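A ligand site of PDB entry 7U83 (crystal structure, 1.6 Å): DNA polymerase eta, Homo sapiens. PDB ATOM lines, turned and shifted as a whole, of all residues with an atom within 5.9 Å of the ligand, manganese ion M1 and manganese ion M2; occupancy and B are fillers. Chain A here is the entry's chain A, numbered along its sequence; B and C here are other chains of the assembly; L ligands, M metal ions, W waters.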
ATOM      1  N   ASP A  16      -2.531  33.688  10.292  1.00  0.00           N
ATOM      2  CA  ASP A  16      -2.130  32.288  10.082  1.00  0.00           C
ATOM      3  C   ASP A  16      -2.210  31.518  11.398  1.00  0.00           C
ATOM      4  O   ASP A  16      -1.600  31.930  12.370  1.00  0.00           O
ATOM      5  CB  ASP A  16      -0.719  32.215   9.525  1.00  0.00           C
ATOM      6  CG  ASP A  16      -0.318  30.809   9.208  1.00  0.00           C
ATOM      7  OD1 ASP A  16      -0.001  30.120  10.152  1.00  0.00           O
ATOM      8  OD2 ASP A  16      -0.380  30.480   8.038  1.00  0.00           O
ATOM      9  N   MET A  17      -2.928  30.403  11.371  1.00  0.00           N
ATOM     10  CA  MET A  17      -3.104  29.664  12.643  1.00  0.00           C
ATOM     11  C   MET A  17      -1.763  29.044  13.080  1.00  0.00           C
ATOM     12  O   MET A  17      -1.036  28.574  12.265  1.00  0.00           O
ATOM     13  CB  MET A  17      -4.180  28.581  12.468  1.00  0.00           C
ATOM     14  CG  MET A  17      -5.467  29.081  11.875  1.00  0.00           C
ATOM     15  SD  MET A  17      -6.177  30.432  12.846  1.00  0.00           S
ATOM     16  CE  MET A  17      -6.510  29.598  14.378  1.00  0.00           C
ATOM     17  N   ASP A  18      -1.484  29.081  14.371  1.00  0.00           N
ATOM     18  CA  ASP A  18      -0.240  28.463  14.850  1.00  0.00           C
ATOM     19  C   ASP A  18      -0.390  26.930  14.832  1.00  0.00           C
ATOM     20  O   ASP A  18      -1.416  26.466  15.294  1.00  0.00           O
ATOM     21  CB  ASP A  18       0.050  28.952  16.260  1.00  0.00           C
ATOM     22  CG  ASP A  18       0.260  30.453  16.374  1.00  0.00           C
ATOM     23  OD1 ASP A  18       0.738  31.051  15.424  1.00  0.00           O
ATOM     24  OD2 ASP A  18      -0.046  30.983  17.439  1.00  0.00           O
ATOM     25  N   CYS A  19       0.641  26.204  14.383  1.00  0.00           N
ATOM     26  CA  CYS A  19       0.633  24.697  14.371  1.00  0.00           C
ATOM     27  C   CYS A  19      -0.810  24.206  14.267  1.00  0.00           C
ATOM     28  O   CYS A  19      -1.213  23.475  15.133  1.00  0.00           O
ATOM     29  CB  CYS A  19       1.442  24.145  15.538  1.00  0.00           C
ATOM     30  SG  CYS A  19       1.029  24.738  17.194  1.00  0.00           S
ATOM     31  N   PHE A  20      -1.472  24.484  13.136  1.00  0.00           N
ATOM     32  CA  PHE A  20      -2.933  24.384  13.094  1.00  0.00           C
ATOM     33  C   PHE A  20      -3.429  22.966  13.399  1.00  0.00           C
ATOM     34  O   PHE A  20      -4.284  22.787  14.293  1.00  0.00           O
ATOM     35  CB  PHE A  20      -3.468  24.865  11.748  1.00  0.00           C
ATOM     36  CG  PHE A  20      -4.978  24.863  11.656  1.00  0.00           C
ATOM     37  CD1 PHE A  20      -5.742  25.410  12.660  1.00  0.00           C
ATOM     38  CD2 PHE A  20      -5.626  24.310  10.565  1.00  0.00           C
ATOM     39  CE1 PHE A  20      -7.169  25.405  12.582  1.00  0.00           C
ATOM     40  CE2 PHE A  20      -7.014  24.296  10.473  1.00  0.00           C
ATOM     41  CZ  PHE A  20      -7.779  24.865  11.468  1.00  0.00           C
ATOM     42  N   PHE A  21      -2.963  21.952  12.655  1.00  0.00           N
ATOM     43  CA  PHE A  21      -3.530  20.625  12.903  1.00  0.00           C
ATOM     44  C   PHE A  21      -3.255  20.158  14.329  1.00  0.00           C
ATOM     45  O   PHE A  21      -4.071  19.447  14.937  1.00  0.00           O
ATOM     46  CB  PHE A  21      -3.016  19.557  11.935  1.00  0.00           C
ATOM     47  CG  PHE A  21      -3.502  19.678  10.501  1.00  0.00           C
ATOM     48  CD1 PHE A  21      -4.096  20.830   9.997  1.00  0.00           C
ATOM     49  CD2 PHE A  21      -3.351  18.586   9.639  1.00  0.00           C
ATOM     50  CE1 PHE A  21      -4.518  20.897   8.639  1.00  0.00           C
ATOM     51  CE2 PHE A  21      -3.778  18.654   8.295  1.00  0.00           C
ATOM     52  CZ  PHE A  21      -4.369  19.803   7.807  1.00  0.00           C
ATOM     53  N   VAL A  22      -2.083  20.542  14.890  1.00  0.00           N
ATOM     54  CA  VAL A  22      -1.810  20.226  16.278  1.00  0.00           C
ATOM     55  C   VAL A  22      -2.842  20.884  17.193  1.00  0.00           C
ATOM     56  O   VAL A  22      -3.352  20.253  18.115  1.00  0.00           O
ATOM     57  CB  VAL A  22      -0.382  20.648  16.648  1.00  0.00           C
ATOM     58  CG1 VAL A  22      -0.209  20.711  18.171  1.00  0.00           C
ATOM     59  CG2 VAL A  22       0.632  19.699  16.023  1.00  0.00           C
ATOM     60  N   GLN A  41       0.636  11.511   9.332  1.00  0.00           N
ATOM     61  CA  GLN A  41      -0.233  10.712   8.487  1.00  0.00           C
ATOM     62  C   GLN A  41       0.366   9.327   8.301  1.00  0.00           C
ATOM     63  O   GLN A  41       1.550   9.205   7.963  1.00  0.00           O
ATOM     64  CB  GLN A  41      -0.558  11.364   7.124  1.00  0.00           C
ATOM     65  CG  GLN A  41      -0.531  12.884   7.098  1.00  0.00           C
ATOM     66  CD  GLN A  41      -0.758  13.453   5.688  1.00  0.00           C
ATOM     67  OE1 GLN A  41      -1.895  13.774   5.322  1.00  0.00           O
ATOM     68  NE2 GLN A  41       0.308  13.577   4.919  1.00  0.00           N
ATOM     69  N   ILE A  51       3.313  16.248   9.675  1.00  0.00           N
ATOM     70  CA  ILE A  51       2.877  17.400   8.892  1.00  0.00           C
ATOM     71  C   ILE A  51       2.653  18.662   9.731  1.00  0.00           C
ATOM     72  O   ILE A  51       2.496  19.742   9.141  1.00  0.00           O
ATOM     73  CB  ILE A  51       1.613  17.095   8.056  1.00  0.00           C
ATOM     74  CG1 ILE A  51       0.452  16.562   8.924  1.00  0.00           C
ATOM     75  CG2 ILE A  51       1.949  16.166   6.897  1.00  0.00           C
ATOM     76  CD1 ILE A  51      -0.855  16.465   8.130  1.00  0.00           C
ATOM     77  N   ALA A  52       2.718  18.586  11.065  1.00  0.00           N
ATOM     78  CA  ALA A  52       2.489  19.746  11.921  1.00  0.00           C
ATOM     79  C   ALA A  52       3.136  19.476  13.269  1.00  0.00           C
ATOM     80  O   ALA A  52       3.100  18.328  13.732  1.00  0.00           O
ATOM     81  CB  ALA A  52       0.992  20.027  12.102  1.00  0.00           C
ATOM     82  N   VAL A  53       3.708  20.524  13.883  1.00  0.00           N
ATOM     83  CA  VAL A  53       4.567  20.363  15.064  1.00  0.00           C
ATOM     84  C   VAL A  53       4.299  21.476  16.075  1.00  0.00           C
ATOM     85  O   VAL A  53       4.396  22.656  15.729  1.00  0.00           O
ATOM     86  CB  VAL A  53       6.056  20.366  14.668  1.00  0.00           C
ATOM     87  CG1 VAL A  53       6.916  20.048  15.863  1.00  0.00           C
ATOM     88  CG2 VAL A  53       6.319  19.354  13.612  1.00  0.00           C
ATOM     89  N   TYR A  55       5.030  24.102  19.122  1.00  0.00           N
ATOM     90  CA  TYR A  55       6.249  24.882  19.349  1.00  0.00           C
ATOM     91  C   TYR A  55       7.160  24.252  20.409  1.00  0.00           C
ATOM     92  O   TYR A  55       8.405  24.329  20.306  1.00  0.00           O
ATOM     93  CB  TYR A  55       5.849  26.323  19.688  1.00  0.00           C
ATOM     94  CG  TYR A  55       5.502  27.042  18.398  1.00  0.00           C
ATOM     95  CD1 TYR A  55       4.278  26.825  17.792  1.00  0.00           C
ATOM     96  CD2 TYR A  55       6.416  27.861  17.750  1.00  0.00           C
ATOM     97  CE1 TYR A  55       3.949  27.443  16.591  1.00  0.00           C
ATOM     98  CE2 TYR A  55       6.104  28.481  16.565  1.00  0.00           C
ATOM     99  CZ  TYR A  55       4.881  28.241  15.967  1.00  0.00           C
ATOM    100  OH  TYR A  55       4.561  28.856  14.770  1.00  0.00           O
ATOM    101  N   ARG A  58       9.089  21.744  18.463  1.00  0.00           N
ATOM    102  CA  ARG A  58      10.054  22.385  17.575  1.00  0.00           C
ATOM    103  C   ARG A  58      11.339  22.722  18.310  1.00  0.00           C
ATOM    104  O   ARG A  58      12.415  22.727  17.689  1.00  0.00           O
ATOM    105  CB  ARG A  58       9.471  23.666  16.984  1.00  0.00           C
ATOM    106  CG  ARG A  58       8.249  23.445  16.140  1.00  0.00           C
ATOM    107  CD  ARG A  58       7.811  24.747  15.520  1.00  0.00           C
ATOM    108  NE  ARG A  58       6.495  24.593  14.910  1.00  0.00           N
ATOM    109  CZ  ARG A  58       5.946  25.450  14.067  1.00  0.00           C
ATOM    110  NH1 ARG A  58       6.587  26.552  13.698  1.00  0.00           N
ATOM    111  NH2 ARG A  58       4.749  25.181  13.543  1.00  0.00           N
ATOM    112  N   ARG A  64       8.215  19.525  10.200  1.00  0.00           N
ATOM    113  CA  ARG A  64       7.378  18.880   9.162  1.00  0.00           C
ATOM    114  C   ARG A  64       8.301  18.109   8.205  1.00  0.00           C
ATOM    115  O   ARG A  64       9.471  18.480   8.096  1.00  0.00           O
ATOM    116  CB  ARG A  64       6.536  19.976   8.483  1.00  0.00           C
ATOM    117  CG  ARG A  64       6.981  20.405   7.101  1.00  0.00           C
ATOM    118  CD  ARG A  64       5.966  21.286   6.402  1.00  0.00           C
ATOM    119  NE  ARG A  64       5.354  20.631   5.261  1.00  0.00           N
ATOM    120  CZ  ARG A  64       5.943  20.413   4.091  1.00  0.00           C
ATOM    121  NH1 ARG A  64       7.185  20.818   3.872  1.00  0.00           N
ATOM    122  NH2 ARG A  64       5.283  19.785   3.129  1.00  0.00           N
ATOM    123  N   LEU A  92      -8.836  14.479   5.664  1.00  0.00           N
ATOM    124  CA  LEU A  92      -8.537  15.698   6.399  1.00  0.00           C
ATOM    125  C   LEU A  92      -9.789  16.492   6.781  1.00  0.00           C
ATOM    126  O   LEU A  92      -9.697  17.703   7.057  1.00  0.00           O
ATOM    127  CB  LEU A  92      -7.561  16.558   5.592  1.00  0.00           C
ATOM    128  CG  LEU A  92      -6.307  15.832   5.100  1.00  0.00           C
ATOM    129  CD1 LEU A  92      -5.479  16.701   4.221  1.00  0.00           C
ATOM    130  CD2 LEU A  92      -5.508  15.332   6.300  1.00  0.00           C
ATOM    131  N   SER A 116      -5.108  29.348   2.288  1.00  0.00           N
ATOM    132  CA  SER A 116      -4.810  27.934   2.605  1.00  0.00           C
ATOM    133  C   SER A 116      -5.829  27.460   3.633  1.00  0.00           C
ATOM    134  O   SER A 116      -6.657  28.241   4.052  1.00  0.00           O
ATOM    135  CB  SER A 116      -3.417  27.777   3.154  1.00  0.00           C
ATOM    136  OG  SER A 116      -3.398  28.034   4.547  1.00  0.00           O
ATOM    137  N   ILE A 117      -5.678  26.226   4.049  1.00  0.00           N
ATOM    138  CA  ILE A 117      -6.550  25.670   5.121  1.00  0.00           C
ATOM    139  C   ILE A 117      -6.385  26.475   6.424  1.00  0.00           C
ATOM    140  O   ILE A 117      -7.291  26.452   7.212  1.00  0.00           O
ATOM    141  CB  ILE A 117      -6.201  24.182   5.348  1.00  0.00           C
ATOM    142  CG1 ILE A 117      -7.325  23.432   6.055  1.00  0.00           C
ATOM    143  CG2 ILE A 117      -4.875  23.992   6.076  1.00  0.00           C
ATOM    144  CD1 ILE A 117      -7.207  21.926   5.944  1.00  0.00           C
ATOM    145  N   ASP A 118      -5.265  27.155   6.596  1.00  0.00           N
ATOM    146  CA  ASP A 118      -5.123  27.817   7.927  1.00  0.00           C
ATOM    147  C   ASP A 118      -4.798  29.315   7.860  1.00  0.00           C
ATOM    148  O   ASP A 118      -4.438  29.882   8.887  1.00  0.00           O
ATOM    149  CB  ASP A 118      -4.154  27.045   8.809  1.00  0.00           C
ATOM    150  CG  ASP A 118      -2.753  27.556   8.717  1.00  0.00           C
ATOM    151  OD1 ASP A 118      -2.352  27.859   7.598  1.00  0.00           O
ATOM    152  OD2 ASP A 118      -2.152  27.669   9.775  1.00  0.00           O
ATOM    153  N   GLU A 119      -4.941  29.922   6.694  1.00  0.00           N
ATOM    154  CA  GLU A 119      -4.621  31.352   6.666  1.00  0.00           C
ATOM    155  C   GLU A 119      -5.458  32.119   5.663  1.00  0.00           C
ATOM    156  O   GLU A 119      -5.906  31.538   4.668  1.00  0.00           O
ATOM    157  CB  GLU A 119      -3.150  31.581   6.369  1.00  0.00           C
ATOM    158  CG  GLU A 119      -2.749  31.364   4.932  1.00  0.00           C
ATOM    159  CD  GLU A 119      -1.335  30.856   4.825  1.00  0.00           C
ATOM    160  OE1 GLU A 119      -1.114  29.667   5.092  1.00  0.00           O
ATOM    161  OE2 GLU A 119      -0.468  31.660   4.528  1.00  0.00           O
ATOM    162  N   LYS A 227       2.399  38.674   4.945  1.00  0.00           N
ATOM    163  CA  LYS A 227       2.774  37.282   5.180  1.00  0.00           C
ATOM    164  C   LYS A 227       4.134  37.188   5.873  1.00  0.00           C
ATOM    165  O   LYS A 227       4.309  36.460   6.880  1.00  0.00           O
ATOM    166  CB  LYS A 227       2.776  36.528   3.846  1.00  0.00           C
ATOM    167  CG  LYS A 227       3.285  35.074   3.918  1.00  0.00           C
ATOM    168  CD  LYS A 227       2.358  34.210   4.792  1.00  0.00           C
ATOM    169  CE  LYS A 227       2.860  32.745   4.846  1.00  0.00           C
ATOM    170  NZ  LYS A 227       1.993  31.824   5.672  1.00  0.00           N
ATOM    171  N   LYS A 234       6.182  34.477  15.684  1.00  0.00           N
ATOM    172  CA  LYS A 234       5.321  33.342  15.959  1.00  0.00           C
ATOM    173  C   LYS A 234       5.870  32.602  17.167  1.00  0.00           C
ATOM    174  O   LYS A 234       7.082  32.539  17.371  1.00  0.00           O
ATOM    175  CB  LYS A 234       5.240  32.395  14.751  1.00  0.00           C
ATOM    176  CG  LYS A 234       4.102  32.684  13.776  1.00  0.00           C
ATOM    177  CD  LYS A 234       3.751  31.456  12.972  1.00  0.00           C
ATOM    178  CE  LYS A 234       2.686  31.738  11.929  1.00  0.00           C
ATOM    179  NZ  LYS A 234       1.403  31.127  12.377  1.00  0.00           N
ATOM    180  N   PRO A 235       4.996  32.036  18.007  1.00  0.00           N
ATOM    181  CA  PRO A 235       3.536  31.967  17.933  1.00  0.00           C
ATOM    182  C   PRO A 235       2.781  32.997  18.751  1.00  0.00           C
ATOM    183  O   PRO A 235       3.342  33.651  19.646  1.00  0.00           O
ATOM    184  CB  PRO A 235       3.246  30.565  18.504  1.00  0.00           C
ATOM    185  CG  PRO A 235       4.267  30.487  19.636  1.00  0.00           C
ATOM    186  CD  PRO A 235       5.520  31.181  19.086  1.00  0.00           C
ATOM    187  P    DT B   3      11.592   9.577   1.055  1.00  0.00           P
ATOM    188  OP1  DT B   3      12.626   9.406   0.022  1.00  0.00           O
ATOM    189  OP2  DT B   3      11.976   9.953   2.432  1.00  0.00           O
ATOM    190  O5'  DT B   3      10.536  10.621   0.486  1.00  0.00           O
ATOM    191  C5'  DT B   3       9.932  11.606   1.341  1.00  0.00           C
ATOM    192  C4'  DT B   3       8.676  11.046   1.968  1.00  0.00           C
ATOM    193  O4'  DT B   3       8.209  11.972   2.986  1.00  0.00           O
ATOM    194  C3'  DT B   3       7.509  10.857   1.000  1.00  0.00           C
ATOM    195  O3'  DT B   3       6.686   9.760   1.397  1.00  0.00           O
ATOM    196  C2'  DT B   3       6.714  12.126   1.206  1.00  0.00           C
ATOM    197  C1'  DT B   3       6.854  12.296   2.702  1.00  0.00           C
ATOM    198  N1   DT B   3       6.635  13.680   3.106  1.00  0.00           N
ATOM    199  C2   DT B   3       5.663  13.974   4.038  1.00  0.00           C
ATOM    200  O2   DT B   3       5.000  13.113   4.603  1.00  0.00           O
ATOM    201  N3   DT B   3       5.503  15.310   4.300  1.00  0.00           N
ATOM    202  C4   DT B   3       6.186  16.365   3.728  1.00  0.00           C
ATOM    203  O4   DT B   3       5.933  17.514   4.065  1.00  0.00           O
ATOM    204  C5   DT B   3       7.184  15.979   2.749  1.00  0.00           C
ATOM    205  C7   DT B   3       7.978  17.049   2.063  1.00  0.00           C
ATOM    206  C6   DT B   3       7.346  14.688   2.486  1.00  0.00           C
ATOM    207  P    DT B   4       5.477   9.284   0.469  1.00  0.00           P
ATOM    208  OP1  DT B   4       5.182   7.875   0.792  1.00  0.00           O
ATOM    209  OP2  DT B   4       5.776   9.681  -0.914  1.00  0.00           O
ATOM    210  O5'  DT B   4       4.263  10.201   0.932  1.00  0.00           O
ATOM    211  C5'  DT B   4       3.738  10.166   2.263  1.00  0.00           C
ATOM    212  C4'  DT B   4       2.507  11.044   2.350  1.00  0.00           C
ATOM    213  O4'  DT B   4       2.888  12.414   2.575  1.00  0.00           O
ATOM    214  C3'  DT B   4       1.635  11.046   1.085  1.00  0.00           C
ATOM    215  O3'  DT B   4       0.323  10.744   1.562  1.00  0.00           O
ATOM    216  C2'  DT B   4       1.817  12.441   0.522  1.00  0.00           C
ATOM    217  C1'  DT B   4       2.127  13.271   1.748  1.00  0.00           C
ATOM    218  N1   DT B   4       2.940  14.472   1.473  1.00  0.00           N
ATOM    219  C2   DT B   4       2.658  15.639   2.144  1.00  0.00           C
ATOM    220  O2   DT B   4       1.742  15.736   2.939  1.00  0.00           O
ATOM    221  N3   DT B   4       3.480  16.685   1.841  1.00  0.00           N
ATOM    222  C4   DT B   4       4.561  16.672   0.968  1.00  0.00           C
ATOM    223  O4   DT B   4       5.186  17.706   0.765  1.00  0.00           O
ATOM    224  C5   DT B   4       4.789  15.426   0.284  1.00  0.00           C
ATOM    225  C7   DT B   4       5.892  15.343  -0.715  1.00  0.00           C
ATOM    226  C6   DT B   4       3.977  14.393   0.576  1.00  0.00           C
ATOM    227  P    DA B   5      -0.904  10.664   0.549  1.00  0.00           P
ATOM    228  OP1  DA B   5      -1.799   9.583   0.991  1.00  0.00           O
ATOM    229  OP2  DA B   5      -0.381  10.628  -0.828  1.00  0.00           O
ATOM    230  O5'  DA B   5      -1.637  12.061   0.760  1.00  0.00           O
ATOM    231  C5'  DA B   5      -2.144  12.446   2.044  1.00  0.00           C
ATOM    232  C4'  DA B   5      -2.835  13.791   1.945  1.00  0.00           C
ATOM    233  O4'  DA B   5      -1.843  14.824   1.762  1.00  0.00           O
ATOM    234  C3'  DA B   5      -3.821  13.942   0.787  1.00  0.00           C
ATOM    235  O3'  DA B   5      -4.947  14.694   1.240  1.00  0.00           O
ATOM    236  C2'  DA B   5      -3.013  14.692  -0.259  1.00  0.00           C
ATOM    237  C1'  DA B   5      -2.130  15.575   0.589  1.00  0.00           C
ATOM    238  N9   DA B   5      -0.864  15.903  -0.048  1.00  0.00           N
ATOM    239  C8   DA B   5      -0.117  15.112  -0.880  1.00  0.00           C
ATOM    240  N7   DA B   5       0.991  15.675  -1.301  1.00  0.00           N
ATOM    241  C5   DA B   5       0.973  16.921  -0.704  1.00  0.00           C
ATOM    242  C6   DA B   5       1.866  18.007  -0.755  1.00  0.00           C
ATOM    243  N6   DA B   5       3.001  17.996  -1.466  1.00  0.00           N
ATOM    244  N1   DA B   5       1.556  19.112  -0.039  1.00  0.00           N
ATOM    245  C2   DA B   5       0.427  19.107   0.674  1.00  0.00           C
ATOM    246  N3   DA B   5      -0.496  18.163   0.791  1.00  0.00           N
ATOM    247  C4   DA B   5      -0.155  17.079   0.073  1.00  0.00           C
ATOM    248  P    DT C   8       5.229  28.159   2.295  1.00  0.00           P
ATOM    249  OP1  DT C   8       4.788  29.350   3.035  1.00  0.00           O
ATOM    250  OP2  DT C   8       6.678  27.896   2.132  1.00  0.00           O
ATOM    251  O5'  DT C   8       4.563  26.855   2.962  1.00  0.00           O
ATOM    252  C5'  DT C   8       3.113  26.566   2.939  1.00  0.00           C
ATOM    253  C4'  DT C   8       2.894  25.101   3.227  1.00  0.00           C
ATOM    254  O4'  DT C   8       3.156  24.287   2.086  1.00  0.00           O
ATOM    255  C3'  DT C   8       3.947  24.694   4.309  1.00  0.00           C
ATOM    256  O3'  DT C   8       3.625  24.067   5.606  1.00  0.00           O
ATOM    257  C2'  DT C   8       4.864  23.753   3.550  1.00  0.00           C
ATOM    258  C1'  DT C   8       3.860  23.193   2.590  1.00  0.00           C
ATOM    259  N1   DT C   8       4.364  22.450   1.466  1.00  0.00           N
ATOM    260  C2   DT C   8       3.454  21.586   0.921  1.00  0.00           C
ATOM    261  O2   DT C   8       2.305  21.509   1.321  1.00  0.00           O
ATOM    262  N3   DT C   8       3.920  20.840  -0.119  1.00  0.00           N
ATOM    263  C4   DT C   8       5.192  20.857  -0.656  1.00  0.00           C
ATOM    264  O4   DT C   8       5.473  20.132  -1.600  1.00  0.00           O
ATOM    265  C5   DT C   8       6.110  21.785  -0.034  1.00  0.00           C
ATOM    266  C7   DT C   8       7.511  21.882  -0.549  1.00  0.00           C
ATOM    267  C6   DT C   8       5.660  22.521   0.991  1.00  0.00           C
HETATM  268  N1  LIG L   1       0.575  17.778   3.715  1.00  0.00           N
HETATM  269  C1  LIG L   1      -0.608  17.923   4.400  1.00  0.00           C
HETATM  270  N2  LIG L   1      -1.515  16.958   4.185  1.00  0.00           N
HETATM  271  N3  LIG L   1      -0.919  18.892   5.251  1.00  0.00           N
HETATM  272  C2  LIG L   1       0.057  19.790   5.414  1.00  0.00           C
HETATM  273  C3  LIG L   1       1.260  19.773   4.802  1.00  0.00           C
HETATM  274  C4  LIG L   1       1.519  18.711   3.924  1.00  0.00           C
HETATM  275  O1  LIG L   1       2.607  18.591   3.344  1.00  0.00           O
HETATM  276  N4  LIG L   1       2.011  20.870   5.206  1.00  0.00           N
HETATM  277  C5  LIG L   1       1.242  21.511   6.058  1.00  0.00           C
HETATM  278  N5  LIG L   1       0.027  20.897   6.220  1.00  0.00           N
HETATM  279  P1  LIG L   1       1.250  25.892   8.066  1.00  0.00           P
HETATM  280  P2  LIG L   1       1.379  25.303  10.960  1.00  0.00           P
HETATM  281  P3  LIG L   1       2.887  27.571  11.907  1.00  0.00           P
HETATM  282  C6  LIG L   1      -1.072  21.242   7.141  1.00  0.00           C
HETATM  283  O2  LIG L   1       0.629  27.203   8.322  1.00  0.00           O
HETATM  284  O3  LIG L   1       0.086  25.993  11.028  1.00  0.00           O
HETATM  285  O4  LIG L   1       4.387  27.660  11.598  1.00  0.00           O
HETATM  286  C7  LIG L   1      -0.711  21.028   8.609  1.00  0.00           C
HETATM  287  O5  LIG L   1       2.399  25.973   6.980  1.00  0.00           O
HETATM  288  O6  LIG L   1       1.326  23.832  11.460  1.00  0.00           O
HETATM  289  O7  LIG L   1       1.992  28.268  10.882  1.00  0.00           O
HETATM  290  C8  LIG L   1      -0.511  22.439   9.140  1.00  0.00           C
HETATM  291  O8  LIG L   1      -0.916  22.471  10.506  1.00  0.00           O
HETATM  292  N6  LIG L   1       1.925  25.252   9.418  1.00  0.00           N
HETATM  293  O9  LIG L   1       2.468  26.044  11.834  1.00  0.00           O
HETATM  294  O10 LIG L   1       2.516  28.004  13.302  1.00  0.00           O
HETATM  295  C9  LIG L   1      -1.442  23.266   8.264  1.00  0.00           C
HETATM  296  O11 LIG L   1      -1.376  22.624   6.969  1.00  0.00           O
HETATM  297  C10 LIG L   1      -1.087  24.725   8.127  1.00  0.00           C
HETATM  298  O12 LIG L   1       0.206  24.848   7.487  1.00  0.00           O
HETATM  299 MN    MN M   1      -0.451  28.576   6.866  1.00  0.00          MN
HETATM  300 MN    MN M   2      -0.099  28.035  10.394  1.00  0.00          MN
HETATM  301  O   HOH W   1       3.685  22.798  12.285  1.00  0.00           O
HETATM  302  O   HOH W   2       1.774  28.941   6.458  1.00  0.00           O
HETATM  303  O   HOH W   3      -0.414  26.984   5.211  1.00  0.00           O
HETATM  304  O   HOH W   4       2.989  29.766   8.770  1.00  0.00           O
HETATM  305  O   HOH W   5       3.388  22.589   8.918  1.00  0.00           O
HETATM  306  O   HOH W   6       5.917  26.038  10.206  1.00  0.00           O
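Lys 234 touches manganese ion M2.
Four residues have an atom within 4 Å of manganese ion M2: Asp 16, Met 17, Asp 118 and Lys 234.
The nearest printed residue that does not touch manganese ion M2 is Asp 18 (4.3 Å).
Water W3 lies within hydrogen-bond range of an oxygen (O12) of the ligand (3.2 Å) and the side-chain hydroxyl of Ser 116 (3.2 Å).
Water W2 bridges NZ of Lys 227 and O5 of the ligand.
Water W1 lies within hydrogen-bond range of an oxygen (O6) of the ligand (2.7 Å), the backbone NH of Val 53 (2.8 Å) and the guanidinium group of Arg 58 (2.9 Å).
Water W5 lies within hydrogen-bond range of O of Ile 51 (3.0 Å) and N6 of the ligand (3.1 Å).
Manganese ion M2 is bound by OD1 of Asp 16 (2.1 Å), O3 of the ligand (2.1 Å), O of Met 17 (2.2 Å), O7 of the ligand (2.2 Å), OD2 of Asp 118 (2.2 Å) and O2 of the ligand (2.3 Å).
Manganese ion M2 has six donor atoms within binding distance.
A nitrogen (N1) of the ligand lies within hydrogen-bond range of O2 of DT 4 of chain B.
O3' of DT 8 of chain C lies close to an oxygen (O5) of the ligand, 2.7 Å away.
The side-chain hydroxyl (OH) of Tyr 55 sits at hydrogen-bond distance from an oxygen (O10) of the ligand.
O10 of the ligand is in hydrogen-bond range of N of Cys 19 (2.8 Å).
O1 of the ligand is in hydrogen-bond range of NH2 of Arg 64, at 2.9 Å.
The guanidinium group of Arg 58 is in salt-bridge range of an oxygen (O4) of the ligand.
The backbone NH (N) of Phe 21 sits at hydrogen-bond distance from an oxygen (O8) of the ligand (3.0 Å).
The backbone NH of Phe 20 lies within hydrogen-bond range of an oxygen (O6) of the ligand (3.3 Å).
O4' of DA 5 of chain B lies within hydrogen-bond range of N2 of the ligand (3.2 Å).
N3 of DA 5 of chain B lies within hydrogen-bond range of N1 of the ligand, 3.1 Å away.
The side-chain amino group of Lys 234 lies within salt-bridge range of an oxygen (O10) of the ligand, at 3.4 Å.
OE1 of Gln 41 sits at hydrogen-bond distance from N2 of the ligand (3.4 Å).
Merely in contact with manganese ion M1: Ser 116 (3.8 Å).
Four residues have an atom within 4 Å of manganese ion M1: Asp 16, Ser 116, Asp 118 and Glu 119.
Along chain A the residues within 4 Å of manganese ion M1 span positions 16 to 119.
Asp 18 touches the ligand.
O of Ile 51 touches C7 of the ligand (3.5 Å).
Ala 52 touches the ligand (CB to O8, 3.5 Å).
Leu 92 touches the ligand (CD1 to N2, 3.97 Å).
CG2 of Ile 117 touches O11 of the ligand, at 3.9 Å.
O4 of DT 3 of chain B touches O1 of the ligand, 3.6 Å away.
Hydrophobic or aromatic side chains within 4 Å of the ligand: Phe 20, Phe 21, Ile 51, Ala 52, Tyr 55, Leu 92 and Ile 117.
The nearest printed residue that does not touch the ligand is Glu 119 (4.4 Å).
Manganese ion M1 is bound by the side-chain carboxylate of Asp 118 (2.2 Å), the side-chain carboxylate of Glu 119 (2.2 Å), the side-chain carboxylate of Asp 16 (2.2 Å), an oxygen (O2) of the ligand (2.3 Å), water W2 (2.3 Å) and water W3 (2.3 Å).
The side-chain amino group of Lys 234 sits at hydrogen-bond distance from the backbone carbonyl oxygen of Asp 16.
OD2 of Asp 16 sits close to NZ of Lys 227 (3.6 Å).
The backbone NH (N) of Asp 118 lies within hydrogen-bond range of the side-chain hydroxyl (OG) of Ser 116 (2.9 Å).
The side-chain carboxylate (OE2) of Glu 119 lies within salt-bridge range of the side-chain amino group (NZ) of Lys 227, at 2.7 Å.
The side-chain hydroxyl of Tyr 55 lies within hydrogen-bond range of the guanidinium group of Arg 58, at 3.2 Å.
The guanidinium group (NH2) of Arg 64 sits at hydrogen-bond distance from O4 of DT 3 of chain B (2.5 Å).
NE of Arg 58 is in hydrogen-bond range of O of Val 53 (3.0 Å).
The side-chain carboxylate of Asp 18 is in salt-bridge range of the side-chain amino group of Lys 234 (3.1 Å).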
